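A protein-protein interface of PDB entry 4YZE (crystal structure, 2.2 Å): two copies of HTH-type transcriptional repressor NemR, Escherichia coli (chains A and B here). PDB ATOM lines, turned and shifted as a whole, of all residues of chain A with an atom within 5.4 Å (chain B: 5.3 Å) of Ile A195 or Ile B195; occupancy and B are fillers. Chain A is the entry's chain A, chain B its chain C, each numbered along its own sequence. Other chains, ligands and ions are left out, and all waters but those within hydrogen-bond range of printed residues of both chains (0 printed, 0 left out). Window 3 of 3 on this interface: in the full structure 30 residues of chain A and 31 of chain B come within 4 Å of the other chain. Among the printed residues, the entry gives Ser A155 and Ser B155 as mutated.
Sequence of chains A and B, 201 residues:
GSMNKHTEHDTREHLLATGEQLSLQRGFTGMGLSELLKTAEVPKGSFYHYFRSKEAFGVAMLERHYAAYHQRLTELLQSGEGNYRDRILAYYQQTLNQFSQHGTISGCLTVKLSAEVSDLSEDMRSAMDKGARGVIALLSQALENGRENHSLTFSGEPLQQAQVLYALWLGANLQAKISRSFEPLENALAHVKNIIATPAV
Of the 11 printed residues of chain A, 4 touch a printed residue of chain B.
Printed residues of chain A that touch a printed residue of chain B: Ser A155, Gln A161, Asn A194 and Ile A195.
Hydrophobic or aromatic side chains of chain A within 4 Å of the printed part of chain B: Ile A195.
Printed residues of chain B that touch a printed residue of chain A: Ser B155, His B191, Asn B194 and Ile B195.
Hydrophobic or aromatic side chains of chain B within 4 Å of the printed part of chain A: His B191 and Ile B195.
Along chain B the printed residues that touch a printed residue of chain A span positions 155 to 195.
Among the printed residues, 4 pairs touch across the chains.
His B191 touches Gln A161.
Ser B155 touches Asn A194 (CB to OD1, 3.6 Å).
CD1 of Ile A195 touches CG1 of Ile B195, at 3.8 Å.
Ile A195 touches just one residue of chain B: Ile B195 (3.8 Å).
Of chain A, only Ile A195 (3.8 Å) comes within 4 Å of Ile B195.
Of the printed residues of chain B, Gln A161 touches His B191 (3.7 Å).
Printed residues of chain A within 4 Å of Asn B194: Ser A155.
Phe A154 touches none of the printed residues of chain B.
Ser A155 touches Asn B194, and with the chains exchanged Asn A194 touches Ser B155.
Gln A161 touches His B191, but with the chains exchanged His A191 does not touch Gln B161 (4.04 Å).
Ile B195 touches its own counterpart, Ile A195.
Positions printed for both chains: 153, 154, 155, 161, 191, 192, 193, 194, 195, 196 and 197.
The side-chain hydroxyl (OG) of Ser A155 is in hydrogen-bond range of the side-chain amide oxygen (OD1) of Asn B194 (2.9 Å).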
ATOM      1  N   THR A 153     -20.011  -0.208 -23.012  1.00  0.00           N
ATOM      2  CA  THR A 153     -18.639  -0.589 -23.295  1.00  0.00           C
ATOM      3  C   THR A 153     -18.538  -2.105 -23.178  1.00  0.00           C
ATOM      4  O   THR A 153     -19.320  -2.723 -22.445  1.00  0.00           O
ATOM      5  CB  THR A 153     -17.638   0.130 -22.337  1.00  0.00           C
ATOM      6  OG1 THR A 153     -16.305   0.020 -22.852  1.00  0.00           O
ATOM      7  CG2 THR A 153     -17.705  -0.443 -20.929  1.00  0.00           C
ATOM      8  N   PHE A 154     -17.607  -2.695 -23.929  1.00  0.00           N
ATOM      9  CA  PHE A 154     -17.327  -4.126 -23.867  1.00  0.00           C
ATOM     10  C   PHE A 154     -15.984  -4.421 -24.525  1.00  0.00           C
ATOM     11  O   PHE A 154     -15.413  -3.567 -25.186  1.00  0.00           O
ATOM     12  CB  PHE A 154     -18.436  -4.941 -24.565  1.00  0.00           C
ATOM     13  CG  PHE A 154     -18.606  -4.610 -26.023  1.00  0.00           C
ATOM     14  CD1 PHE A 154     -19.455  -3.586 -26.422  1.00  0.00           C
ATOM     15  CD2 PHE A 154     -17.916  -5.324 -27.000  1.00  0.00           C
ATOM     16  CE1 PHE A 154     -19.616  -3.274 -27.772  1.00  0.00           C
ATOM     17  CE2 PHE A 154     -18.060  -5.017 -28.353  1.00  0.00           C
ATOM     18  CZ  PHE A 154     -18.917  -3.993 -28.739  1.00  0.00           C
ATOM     19  N   SER A 155     -15.507  -5.656 -24.386  1.00  0.00           N
ATOM     20  CA  SER A 155     -14.244  -6.068 -24.988  1.00  0.00           C
ATOM     21  C   SER A 155     -14.411  -6.566 -26.425  1.00  0.00           C
ATOM     22  O   SER A 155     -15.281  -7.391 -26.701  1.00  0.00           O
ATOM     23  CB  SER A 155     -13.603  -7.164 -24.132  1.00  0.00           C
ATOM     24  OG  SER A 155     -12.257  -7.396 -24.506  1.00  0.00           O
ATOM     25  N   GLN A 161     -18.652  -9.949 -30.525  1.00  0.00           N
ATOM     26  CA  GLN A 161     -19.424  -9.889 -29.292  1.00  0.00           C
ATOM     27  C   GLN A 161     -20.873 -10.226 -29.584  1.00  0.00           C
ATOM     28  O   GLN A 161     -21.519 -10.885 -28.779  1.00  0.00           O
ATOM     29  CB  GLN A 161     -19.289  -8.523 -28.594  1.00  0.00           C
ATOM     30  CG  GLN A 161     -20.200  -8.365 -27.375  1.00  0.00           C
ATOM     31  CD  GLN A 161     -19.890  -9.365 -26.261  1.00  0.00           C
ATOM     32  OE1 GLN A 161     -20.676 -10.288 -25.983  1.00  0.00           O
ATOM     33  NE2 GLN A 161     -18.749  -9.184 -25.619  1.00  0.00           N
ATOM     34  N   HIS A 191     -25.311 -11.951 -16.615  1.00  0.00           N
ATOM     35  CA  HIS A 191     -23.946 -11.927 -17.140  1.00  0.00           C
ATOM     36  C   HIS A 191     -23.779 -10.877 -18.258  1.00  0.00           C
ATOM     37  O   HIS A 191     -22.744 -10.181 -18.325  1.00  0.00           O
ATOM     38  CB  HIS A 191     -23.502 -13.327 -17.554  1.00  0.00           C
ATOM     39  CG  HIS A 191     -22.201 -13.378 -18.295  1.00  0.00           C
ATOM     40  ND1 HIS A 191     -20.982 -13.489 -17.660  1.00  0.00           N
ATOM     41  CD2 HIS A 191     -21.936 -13.393 -19.622  1.00  0.00           C
ATOM     42  CE1 HIS A 191     -20.019 -13.542 -18.564  1.00  0.00           C
ATOM     43  NE2 HIS A 191     -20.572 -13.490 -19.765  1.00  0.00           N
ATOM     44  N   VAL A 192     -24.801 -10.733 -19.100  1.00  0.00           N
ATOM     45  CA  VAL A 192     -24.796  -9.680 -20.115  1.00  0.00           C
ATOM     46  C   VAL A 192     -24.708  -8.282 -19.481  1.00  0.00           C
ATOM     47  O   VAL A 192     -23.971  -7.407 -19.975  1.00  0.00           O
ATOM     48  CB  VAL A 192     -26.027  -9.776 -21.025  1.00  0.00           C
ATOM     49  CG1 VAL A 192     -26.080  -8.599 -21.989  1.00  0.00           C
ATOM     50  CG2 VAL A 192     -26.022 -11.103 -21.799  1.00  0.00           C
ATOM     51  N   LYS A 193     -25.457  -8.077 -18.394  1.00  0.00           N
ATOM     52  CA  LYS A 193     -25.422  -6.807 -17.656  1.00  0.00           C
ATOM     53  C   LYS A 193     -24.015  -6.440 -17.235  1.00  0.00           C
ATOM     54  O   LYS A 193     -23.664  -5.263 -17.180  1.00  0.00           O
ATOM     55  CB  LYS A 193     -26.290  -6.876 -16.401  1.00  0.00           C
ATOM     56  CG  LYS A 193     -27.754  -6.530 -16.626  1.00  0.00           C
ATOM     57  CD  LYS A 193     -28.570  -6.696 -15.341  1.00  0.00           C
ATOM     58  CE  LYS A 193     -30.047  -6.476 -15.622  1.00  0.00           C
ATOM     59  NZ  LYS A 193     -30.915  -6.913 -14.490  1.00  0.00           N
ATOM     60  N   ASN A 194     -23.207  -7.447 -16.930  1.00  0.00           N
ATOM     61  CA  ASN A 194     -21.846  -7.197 -16.472  1.00  0.00           C
ATOM     62  C   ASN A 194     -20.863  -7.056 -17.646  1.00  0.00           C
ATOM     63  O   ASN A 194     -19.895  -6.312 -17.572  1.00  0.00           O
ATOM     64  CB  ASN A 194     -21.409  -8.313 -15.519  1.00  0.00           C
ATOM     65  CG  ASN A 194     -20.155  -7.964 -14.745  1.00  0.00           C
ATOM     66  OD1 ASN A 194     -19.086  -8.535 -14.977  1.00  0.00           O
ATOM     67  ND2 ASN A 194     -20.277  -7.014 -13.821  1.00  0.00           N
ATOM     68  N   ILE A 195     -21.131  -7.766 -18.737  1.00  0.00           N
ATOM     69  CA  ILE A 195     -20.236  -7.775 -19.893  1.00  0.00           C
ATOM     70  C   ILE A 195     -20.432  -6.532 -20.762  1.00  0.00           C
ATOM     71  O   ILE A 195     -19.461  -5.935 -21.233  1.00  0.00           O
ATOM     72  CB  ILE A 195     -20.439  -9.063 -20.735  1.00  0.00           C
ATOM     73  CG1 ILE A 195     -19.928 -10.275 -19.960  1.00  0.00           C
ATOM     74  CG2 ILE A 195     -19.710  -8.964 -22.046  1.00  0.00           C
ATOM     75  CD1 ILE A 195     -18.531 -10.055 -19.385  1.00  0.00           C
ATOM     76  N   ILE A 196     -21.695  -6.176 -21.000  1.00  0.00           N
ATOM     77  CA  ILE A 196     -22.048  -4.972 -21.746  1.00  0.00           C
ATOM     78  C   ILE A 196     -22.356  -3.918 -20.695  1.00  0.00           C
ATOM     79  O   ILE A 196     -23.500  -3.811 -20.237  1.00  0.00           O
ATOM     80  CB  ILE A 196     -23.295  -5.191 -22.663  1.00  0.00           C
ATOM     81  CG1 ILE A 196     -23.119  -6.435 -23.531  1.00  0.00           C
ATOM     82  CG2 ILE A 196     -23.558  -3.948 -23.533  1.00  0.00           C
ATOM     83  CD1 ILE A 196     -21.881  -6.428 -24.430  1.00  0.00           C
ATOM     84  N   ALA A 197     -21.330  -3.163 -20.295  1.00  0.00           N
ATOM     85  CA  ALA A 197     -21.430  -2.281 -19.129  1.00  0.00           C
ATOM     86  C   ALA A 197     -21.738  -0.846 -19.493  1.00  0.00           C
ATOM     87  O   ALA A 197     -21.550  -0.414 -20.628  1.00  0.00           O
ATOM     88  CB  ALA A 197     -20.147  -2.326 -18.299  1.00  0.00           C
ATOM     89  N   THR B 153      -8.506 -15.040 -13.357  1.00  0.00           N
ATOM     90  CA  THR B 153      -9.492 -14.235 -12.649  1.00  0.00           C
ATOM     91  C   THR B 153     -10.723 -14.003 -13.518  1.00  0.00           C
ATOM     92  O   THR B 153     -10.644 -14.003 -14.751  1.00  0.00           O
ATOM     93  CB  THR B 153      -8.918 -12.863 -12.234  1.00  0.00           C
ATOM     94  OG1 THR B 153      -9.889 -12.154 -11.449  1.00  0.00           O
ATOM     95  CG2 THR B 153      -8.551 -12.049 -13.462  1.00  0.00           C
ATOM     96  N   PHE B 154     -11.863 -13.805 -12.864  1.00  0.00           N
ATOM     97  CA  PHE B 154     -13.112 -13.525 -13.560  1.00  0.00           C
ATOM     98  C   PHE B 154     -14.025 -12.814 -12.562  1.00  0.00           C
ATOM     99  O   PHE B 154     -13.723 -12.779 -11.372  1.00  0.00           O
ATOM    100  CB  PHE B 154     -13.757 -14.828 -14.074  1.00  0.00           C
ATOM    101  CG  PHE B 154     -14.006 -15.844 -12.988  1.00  0.00           C
ATOM    102  CD1 PHE B 154     -13.000 -16.724 -12.603  1.00  0.00           C
ATOM    103  CD2 PHE B 154     -15.230 -15.903 -12.334  1.00  0.00           C
ATOM    104  CE1 PHE B 154     -13.205 -17.643 -11.592  1.00  0.00           C
ATOM    105  CE2 PHE B 154     -15.445 -16.823 -11.318  1.00  0.00           C
ATOM    106  CZ  PHE B 154     -14.430 -17.697 -10.949  1.00  0.00           C
ATOM    107  N   SER B 155     -15.141 -12.261 -13.037  1.00  0.00           N
ATOM    108  CA  SER B 155     -16.108 -11.590 -12.167  1.00  0.00           C
ATOM    109  C   SER B 155     -17.201 -12.533 -11.644  1.00  0.00           C
ATOM    110  O   SER B 155     -17.709 -13.382 -12.389  1.00  0.00           O
ATOM    111  CB  SER B 155     -16.758 -10.428 -12.919  1.00  0.00           C
ATOM    112  OG  SER B 155     -15.804  -9.445 -13.260  1.00  0.00           O
ATOM    113  N   GLN B 161     -20.533 -18.421 -13.284  1.00  0.00           N
ATOM    114  CA  GLN B 161     -19.640 -18.287 -14.426  1.00  0.00           C
ATOM    115  C   GLN B 161     -19.539 -19.616 -15.184  1.00  0.00           C
ATOM    116  O   GLN B 161     -19.504 -19.632 -16.417  1.00  0.00           O
ATOM    117  CB  GLN B 161     -18.255 -17.810 -13.966  1.00  0.00           C
ATOM    118  CG  GLN B 161     -17.245 -17.635 -15.106  1.00  0.00           C
ATOM    119  CD  GLN B 161     -17.659 -16.554 -16.098  1.00  0.00           C
ATOM    120  OE1 GLN B 161     -18.135 -16.846 -17.206  1.00  0.00           O
ATOM    121  NE2 GLN B 161     -17.488 -15.301 -15.703  1.00  0.00           N
ATOM    122  N   HIS B 191     -13.700 -15.192 -26.871  1.00  0.00           N
ATOM    123  CA  HIS B 191     -14.424 -14.475 -25.822  1.00  0.00           C
ATOM    124  C   HIS B 191     -13.996 -14.966 -24.440  1.00  0.00           C
ATOM    125  O   HIS B 191     -13.778 -14.151 -23.532  1.00  0.00           O
ATOM    126  CB  HIS B 191     -15.943 -14.613 -25.995  1.00  0.00           C
ATOM    127  CG  HIS B 191     -16.752 -13.805 -25.021  1.00  0.00           C
ATOM    128  ND1 HIS B 191     -17.385 -14.368 -23.930  1.00  0.00           N
ATOM    129  CD2 HIS B 191     -17.048 -12.484 -24.986  1.00  0.00           C
ATOM    130  CE1 HIS B 191     -18.032 -13.426 -23.263  1.00  0.00           C
ATOM    131  NE2 HIS B 191     -17.844 -12.274 -23.883  1.00  0.00           N
ATOM    132  N   VAL B 192     -13.877 -16.287 -24.286  1.00  0.00           N
ATOM    133  CA  VAL B 192     -13.538 -16.886 -22.988  1.00  0.00           C
ATOM    134  C   VAL B 192     -12.131 -16.472 -22.517  1.00  0.00           C
ATOM    135  O   VAL B 192     -11.859 -16.377 -21.309  1.00  0.00           O
ATOM    136  CB  VAL B 192     -13.692 -18.421 -23.033  1.00  0.00           C
ATOM    137  CG1 VAL B 192     -13.114 -19.096 -21.796  1.00  0.00           C
ATOM    138  CG2 VAL B 192     -15.145 -18.782 -23.185  1.00  0.00           C
ATOM    139  N   LYS B 193     -11.246 -16.204 -23.473  1.00  0.00           N
ATOM    140  CA  LYS B 193      -9.908 -15.742 -23.131  1.00  0.00           C
ATOM    141  C   LYS B 193      -9.921 -14.377 -22.433  1.00  0.00           C
ATOM    142  O   LYS B 193      -9.123 -14.158 -21.535  1.00  0.00           O
ATOM    143  CB  LYS B 193      -8.977 -15.756 -24.351  1.00  0.00           C
ATOM    144  CG  LYS B 193      -8.506 -17.163 -24.702  1.00  0.00           C
ATOM    145  CD  LYS B 193      -7.800 -17.228 -26.063  1.00  0.00           C
ATOM    146  CE  LYS B 193      -7.396 -18.665 -26.396  1.00  0.00           C
ATOM    147  NZ  LYS B 193      -6.816 -18.825 -27.766  1.00  0.00           N
ATOM    148  N   ASN B 194     -10.838 -13.491 -22.823  1.00  0.00           N
ATOM    149  CA  ASN B 194     -11.021 -12.212 -22.131  1.00  0.00           C
ATOM    150  C   ASN B 194     -11.638 -12.402 -20.754  1.00  0.00           C
ATOM    151  O   ASN B 194     -11.138 -11.899 -19.752  1.00  0.00           O
ATOM    152  CB  ASN B 194     -11.943 -11.282 -22.925  1.00  0.00           C
ATOM    153  CG  ASN B 194     -11.369 -10.876 -24.256  1.00  0.00           C
ATOM    154  OD1 ASN B 194     -12.035 -10.213 -25.048  1.00  0.00           O
ATOM    155  ND2 ASN B 194     -10.132 -11.267 -24.516  1.00  0.00           N
ATOM    156  N   ILE B 195     -12.743 -13.132 -20.719  1.00  0.00           N
ATOM    157  CA  ILE B 195     -13.536 -13.266 -19.509  1.00  0.00           C
ATOM    158  C   ILE B 195     -12.814 -14.087 -18.441  1.00  0.00           C
ATOM    159  O   ILE B 195     -12.925 -13.804 -17.249  1.00  0.00           O
ATOM    160  CB  ILE B 195     -14.932 -13.848 -19.827  1.00  0.00           C
ATOM    161  CG1 ILE B 195     -15.912 -12.727 -20.189  1.00  0.00           C
ATOM    162  CG2 ILE B 195     -15.487 -14.622 -18.655  1.00  0.00           C
ATOM    163  CD1 ILE B 195     -15.545 -11.932 -21.424  1.00  0.00           C
ATOM    164  N   ILE B 196     -12.073 -15.100 -18.864  1.00  0.00           N
ATOM    165  CA  ILE B 196     -11.309 -15.899 -17.919  1.00  0.00           C
ATOM    166  C   ILE B 196      -9.860 -15.518 -18.123  1.00  0.00           C
ATOM    167  O   ILE B 196      -9.138 -16.189 -18.866  1.00  0.00           O
ATOM    168  CB  ILE B 196     -11.494 -17.401 -18.161  1.00  0.00           C
ATOM    169  CG1 ILE B 196     -12.978 -17.721 -18.335  1.00  0.00           C
ATOM    170  CG2 ILE B 196     -10.892 -18.206 -17.010  1.00  0.00           C
ATOM    171  CD1 ILE B 196     -13.823 -17.399 -17.125  1.00  0.00           C
ATOM    172  N   ALA B 197      -9.437 -14.435 -17.466  1.00  0.00           N
ATOM    173  CA  ALA B 197      -8.189 -13.773 -17.832  1.00  0.00           C
ATOM    174  C   ALA B 197      -7.004 -14.184 -16.969  1.00  0.00           C
ATOM    175  O   ALA B 197      -7.159 -14.536 -15.804  1.00  0.00           O
ATOM    176  CB  ALA B 197      -8.360 -12.246 -17.816  1.00  0.00           C
